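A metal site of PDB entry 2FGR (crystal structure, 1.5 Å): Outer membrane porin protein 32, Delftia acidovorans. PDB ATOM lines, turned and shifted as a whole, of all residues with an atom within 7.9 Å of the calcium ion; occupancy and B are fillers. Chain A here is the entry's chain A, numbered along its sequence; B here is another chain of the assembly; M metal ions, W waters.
Within 4 Å of the calcium ion: Leu 29, Asp 64, Gly 309, Asn 136 of chain B and Glu 158 of chain B.
O of Asn 136 of chain B lies within hydrogen-bond range of N of Phe 156 of chain B, at 3.1 Å.
The calcium ion is bound by O of Gly 309, OD2 of Asp 64, OD1 of Asn 136 of chain B, O of Leu 29, water W1, OE2 of Glu 158 of chain B and OE1 of Glu 158 of chain B.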
ATOM      1  N   ASN A  13      -3.932 -20.757   0.405  1.00  0.00           N
ATOM      2  CA  ASN A  13      -3.974 -22.053  -0.281  1.00  0.00           C
ATOM      3  C   ASN A  13      -4.409 -21.871  -1.718  1.00  0.00           C
ATOM      4  O   ASN A  13      -4.938 -20.831  -2.101  1.00  0.00           O
ATOM      5  CB  ASN A  13      -4.878 -23.062   0.412  1.00  0.00           C
ATOM      6  CG  ASN A  13      -6.309 -22.557   0.645  1.00  0.00           C
ATOM      7  OD1 ASN A  13      -6.999 -22.151  -0.294  1.00  0.00           O
ATOM      8  ND2 ASN A  13      -6.750 -22.562   1.917  1.00  0.00           N
ATOM      9  N   TYR A  27     -11.824 -23.093  -9.115  1.00  0.00           N
ATOM     10  CA  TYR A  27     -10.535 -23.191  -8.484  1.00  0.00           C
ATOM     11  C   TYR A  27      -9.952 -21.799  -8.318  1.00  0.00           C
ATOM     12  O   TYR A  27     -10.377 -20.849  -8.974  1.00  0.00           O
ATOM     13  CB  TYR A  27      -9.627 -24.118  -9.244  1.00  0.00           C
ATOM     14  CG  TYR A  27      -9.328 -23.632 -10.629  1.00  0.00           C
ATOM     15  CD1 TYR A  27      -8.224 -22.860 -10.876  1.00  0.00           C
ATOM     16  CD2 TYR A  27     -10.185 -23.942 -11.687  1.00  0.00           C
ATOM     17  CE1 TYR A  27      -7.920 -22.395 -12.137  1.00  0.00           C
ATOM     18  CE2 TYR A  27      -9.908 -23.444 -12.993  1.00  0.00           C
ATOM     19  CZ  TYR A  27      -8.771 -22.675 -13.197  1.00  0.00           C
ATOM     20  OH  TYR A  27      -8.442 -22.173 -14.452  1.00  0.00           O
ATOM     21  N   GLY A  28      -9.028 -21.680  -7.380  1.00  0.00           N
ATOM     22  CA  GLY A  28      -8.503 -20.380  -7.122  1.00  0.00           C
ATOM     23  C   GLY A  28      -7.592 -20.355  -5.914  1.00  0.00           C
ATOM     24  O   GLY A  28      -7.092 -21.365  -5.494  1.00  0.00           O
ATOM     25  N   LEU A  29      -7.315 -19.159  -5.447  1.00  0.00           N
ATOM     26  CA  LEU A  29      -6.479 -18.926  -4.256  1.00  0.00           C
ATOM     27  C   LEU A  29      -7.450 -18.629  -3.141  1.00  0.00           C
ATOM     28  O   LEU A  29      -8.229 -17.684  -3.214  1.00  0.00           O
ATOM     29  CB  LEU A  29      -5.552 -17.724  -4.473  1.00  0.00           C
ATOM     30  CG  LEU A  29      -4.364 -17.725  -3.476  1.00  0.00           C
ATOM     31  CD1 LEU A  29      -3.260 -18.683  -3.905  1.00  0.00           C
ATOM     32  CD2 LEU A  29      -3.791 -16.323  -3.329  1.00  0.00           C
ATOM     33  N   GLY A  30      -7.398 -19.436  -2.107  1.00  0.00           N
ATOM     34  CA  GLY A  30      -8.241 -19.233  -0.934  1.00  0.00           C
ATOM     35  C   GLY A  30      -7.410 -19.085   0.319  1.00  0.00           C
ATOM     36  O   GLY A  30      -6.200 -18.890   0.279  1.00  0.00           O
ATOM     37  N   THR A  31      -8.073 -19.199   1.464  1.00  0.00           N
ATOM     38  CA  THR A  31      -7.470 -18.948   2.751  1.00  0.00           C
ATOM     39  C   THR A  31      -7.909 -19.919   3.797  1.00  0.00           C
ATOM     40  O   THR A  31      -8.961 -20.603   3.668  1.00  0.00           O
ATOM     41  CB  THR A  31      -7.745 -17.519   3.274  1.00  0.00           C
ATOM     42  OG1 THR A  31      -9.141 -17.314   3.451  1.00  0.00           O
ATOM     43  CG2 THR A  31      -7.314 -16.483   2.258  1.00  0.00           C
ATOM     44  N   GLY A  63      -5.901 -13.235   2.962  1.00  0.00           N
ATOM     45  CA  GLY A  63      -4.696 -12.911   2.201  1.00  0.00           C
ATOM     46  C   GLY A  63      -4.890 -12.917   0.708  1.00  0.00           C
ATOM     47  O   GLY A  63      -4.154 -12.258  -0.030  1.00  0.00           O
ATOM     48  N   ASP A  64      -5.919 -13.589   0.215  1.00  0.00           N
ATOM     49  CA  ASP A  64      -6.152 -13.581  -1.210  1.00  0.00           C
ATOM     50  C   ASP A  64      -6.663 -12.244  -1.763  1.00  0.00           C
ATOM     51  O   ASP A  64      -6.500 -11.966  -2.936  1.00  0.00           O
ATOM     52  CB  ASP A  64      -7.069 -14.726  -1.678  1.00  0.00           C
ATOM     53  CG  ASP A  64      -8.448 -14.718  -1.052  1.00  0.00           C
ATOM     54  OD1 ASP A  64      -8.667 -14.138   0.059  1.00  0.00           O
ATOM     55  OD2 ASP A  64      -9.424 -15.299  -1.652  1.00  0.00           O
ATOM     56  N   ASP A  65      -7.288 -11.410  -0.928  1.00  0.00           N
ATOM     57  CA  ASP A  65      -7.811 -10.111  -1.374  1.00  0.00           C
ATOM     58  C   ASP A  65      -7.430  -8.931  -0.517  1.00  0.00           C
ATOM     59  O   ASP A  65      -7.944  -7.825  -0.695  1.00  0.00           O
ATOM     60  CB  ASP A  65      -9.300 -10.165  -1.653  1.00  0.00           C
ATOM     61  CG  ASP A  65     -10.164 -10.251  -0.442  1.00  0.00           C
ATOM     62  OD1 ASP A  65      -9.743  -9.974   0.724  1.00  0.00           O
ATOM     63  OD2 ASP A  65     -11.384 -10.534  -0.601  1.00  0.00           O
ATOM     64  N   ALA A 307     -14.596 -24.069   0.849  1.00  0.00           N
ATOM     65  CA  ALA A 307     -13.287 -23.632   0.334  1.00  0.00           C
ATOM     66  C   ALA A 307     -13.230 -22.099   0.392  1.00  0.00           C
ATOM     67  O   ALA A 307     -13.512 -21.434  -0.591  1.00  0.00           O
ATOM     68  CB  ALA A 307     -13.049 -24.120  -1.078  1.00  0.00           C
ATOM     69  N   LYS A 308     -12.895 -21.588   1.565  1.00  0.00           N
ATOM     70  CA  LYS A 308     -12.975 -20.165   1.802  1.00  0.00           C
ATOM     71  C   LYS A 308     -12.082 -19.418   0.807  1.00  0.00           C
ATOM     72  O   LYS A 308     -10.925 -19.769   0.619  1.00  0.00           O
ATOM     73  CB  LYS A 308     -12.558 -19.813   3.209  1.00  0.00           C
ATOM     74  CG  LYS A 308     -12.654 -18.348   3.522  1.00  0.00           C
ATOM     75  CD  LYS A 308     -12.361 -18.088   4.993  1.00  0.00           C
ATOM     76  CE  LYS A 308     -13.623 -18.308   5.853  1.00  0.00           C
ATOM     77  NZ  LYS A 308     -13.399 -18.128   7.302  1.00  0.00           N
ATOM     78  N   GLY A 309     -12.647 -18.425   0.179  1.00  0.00           N
ATOM     79  CA  GLY A 309     -11.958 -17.625  -0.815  1.00  0.00           C
ATOM     80  C   GLY A 309     -11.986 -18.180  -2.214  1.00  0.00           C
ATOM     81  O   GLY A 309     -11.462 -17.543  -3.115  1.00  0.00           O
ATOM     82  N   VAL A 310     -12.594 -19.345  -2.419  1.00  0.00           N
ATOM     83  CA  VAL A 310     -12.718 -19.926  -3.762  1.00  0.00           C
ATOM     84  C   VAL A 310     -14.180 -20.199  -4.025  1.00  0.00           C
ATOM     85  O   VAL A 310     -14.758 -19.596  -4.906  1.00  0.00           O
ATOM     86  CB  VAL A 310     -11.858 -21.166  -3.919  1.00  0.00           C
ATOM     87  CG1 VAL A 310     -12.099 -21.800  -5.317  1.00  0.00           C
ATOM     88  CG2 VAL A 310     -10.375 -20.770  -3.834  1.00  0.00           C
ATOM     89  N   TYR A 311     -14.774 -21.109  -3.234  1.00  0.00           N
ATOM     90  CA  TYR A 311     -16.222 -21.380  -3.326  1.00  0.00           C
ATOM     91  C   TYR A 311     -16.698 -22.045  -2.063  1.00  0.00           C
ATOM     92  O   TYR A 311     -16.142 -23.044  -1.637  1.00  0.00           O
ATOM     93  CB  TYR A 311     -16.553 -22.247  -4.574  1.00  0.00           C
ATOM     94  CG  TYR A 311     -18.064 -22.429  -4.733  1.00  0.00           C
ATOM     95  CD1 TYR A 311     -18.872 -21.374  -5.138  1.00  0.00           C
ATOM     96  CD2 TYR A 311     -18.693 -23.607  -4.361  1.00  0.00           C
ATOM     97  CE1 TYR A 311     -20.245 -21.508  -5.240  1.00  0.00           C
ATOM     98  CE2 TYR A 311     -20.081 -23.746  -4.459  1.00  0.00           C
ATOM     99  CZ  TYR A 311     -20.846 -22.694  -4.898  1.00  0.00           C
ATOM    100  OH  TYR A 311     -22.227 -22.793  -4.977  1.00  0.00           O
ATOM    101  N   ASN B 135      -5.809  -9.570  -6.940  1.00  0.00           N
ATOM    102  CA  ASN B 135      -6.271 -10.587  -6.005  1.00  0.00           C
ATOM    103  C   ASN B 135      -5.845 -11.978  -6.437  1.00  0.00           C
ATOM    104  O   ASN B 135      -5.632 -12.236  -7.632  1.00  0.00           O
ATOM    105  CB  ASN B 135      -7.818 -10.553  -5.913  1.00  0.00           C
ATOM    106  CG  ASN B 135      -8.360  -9.261  -5.374  1.00  0.00           C
ATOM    107  OD1 ASN B 135      -9.453  -8.765  -5.800  1.00  0.00           O
ATOM    108  ND2 ASN B 135      -7.661  -8.689  -4.497  1.00  0.00           N
ATOM    109  N   ASN B 136      -5.765 -12.925  -5.522  1.00  0.00           N
ATOM    110  CA  ASN B 136      -5.650 -14.316  -5.887  1.00  0.00           C
ATOM    111  C   ASN B 136      -4.353 -14.627  -6.648  1.00  0.00           C
ATOM    112  O   ASN B 136      -4.330 -15.513  -7.513  1.00  0.00           O
ATOM    113  CB  ASN B 136      -6.862 -14.797  -6.713  1.00  0.00           C
ATOM    114  CG  ASN B 136      -8.184 -14.397  -6.044  1.00  0.00           C
ATOM    115  OD1 ASN B 136      -8.335 -14.601  -4.833  1.00  0.00           O
ATOM    116  ND2 ASN B 136      -9.110 -13.804  -6.818  1.00  0.00           N
ATOM    117  N   LEU B 137      -3.290 -13.933  -6.281  1.00  0.00           N
ATOM    118  CA  LEU B 137      -2.026 -13.955  -6.993  1.00  0.00           C
ATOM    119  C   LEU B 137      -1.015 -14.946  -6.438  1.00  0.00           C
ATOM    120  O   LEU B 137      -0.824 -15.055  -5.204  1.00  0.00           O
ATOM    121  CB  LEU B 137      -1.437 -12.547  -6.967  1.00  0.00           C
ATOM    122  CG  LEU B 137      -0.091 -12.327  -7.637  1.00  0.00           C
ATOM    123  CD1 LEU B 137      -0.164 -12.534  -9.147  1.00  0.00           C
ATOM    124  CD2 LEU B 137       0.374 -10.937  -7.315  1.00  0.00           C
ATOM    125  N   PHE B 156      -5.708 -16.015 -10.270  1.00  0.00           N
ATOM    126  CA  PHE B 156      -6.930 -16.741 -10.557  1.00  0.00           C
ATOM    127  C   PHE B 156      -8.121 -15.816 -10.674  1.00  0.00           C
ATOM    128  O   PHE B 156      -8.355 -14.978  -9.803  1.00  0.00           O
ATOM    129  CB  PHE B 156      -7.233 -17.777  -9.479  1.00  0.00           C
ATOM    130  CG  PHE B 156      -6.195 -18.830  -9.317  1.00  0.00           C
ATOM    131  CD1 PHE B 156      -5.185 -18.678  -8.396  1.00  0.00           C
ATOM    132  CD2 PHE B 156      -6.213 -19.996 -10.087  1.00  0.00           C
ATOM    133  CE1 PHE B 156      -4.215 -19.676  -8.225  1.00  0.00           C
ATOM    134  CE2 PHE B 156      -5.260 -20.969  -9.920  1.00  0.00           C
ATOM    135  CZ  PHE B 156      -4.255 -20.815  -8.991  1.00  0.00           C
ATOM    136  N   ASP B 157      -8.932 -16.010 -11.719  1.00  0.00           N
ATOM    137  CA  ASP B 157     -10.192 -15.279 -11.869  1.00  0.00           C
ATOM    138  C   ASP B 157     -11.310 -15.786 -11.007  1.00  0.00           C
ATOM    139  O   ASP B 157     -12.209 -15.022 -10.653  1.00  0.00           O
ATOM    140  CB  ASP B 157     -10.660 -15.338 -13.332  1.00  0.00           C
ATOM    141  CG  ASP B 157     -10.658 -16.742 -13.864  1.00  0.00           C
ATOM    142  OD1 ASP B 157     -11.727 -17.409 -13.842  1.00  0.00           O
ATOM    143  OD2 ASP B 157      -9.593 -17.308 -14.247  1.00  0.00           O
ATOM    144  N   GLU B 158     -11.259 -17.070 -10.693  1.00  0.00           N
ATOM    145  CA  GLU B 158     -12.272 -17.723  -9.846  1.00  0.00           C
ATOM    146  C   GLU B 158     -13.690 -17.551 -10.401  1.00  0.00           C
ATOM    147  O   GLU B 158     -14.672 -17.450  -9.649  1.00  0.00           O
ATOM    148  CB  GLU B 158     -12.176 -17.219  -8.398  1.00  0.00           C
ATOM    149  CG  GLU B 158     -10.780 -17.368  -7.859  1.00  0.00           C
ATOM    150  CD  GLU B 158     -10.531 -16.887  -6.436  1.00  0.00           C
ATOM    151  OE1 GLU B 158     -11.328 -16.111  -5.839  1.00  0.00           O
ATOM    152  OE2 GLU B 158      -9.450 -17.270  -5.923  1.00  0.00           O
HETATM  153 CA    CA M   1      -9.846 -16.068  -3.816  1.00  0.00          CA
HETATM  154  O   HOH W   1     -11.428 -14.244  -3.528  1.00  0.00           O
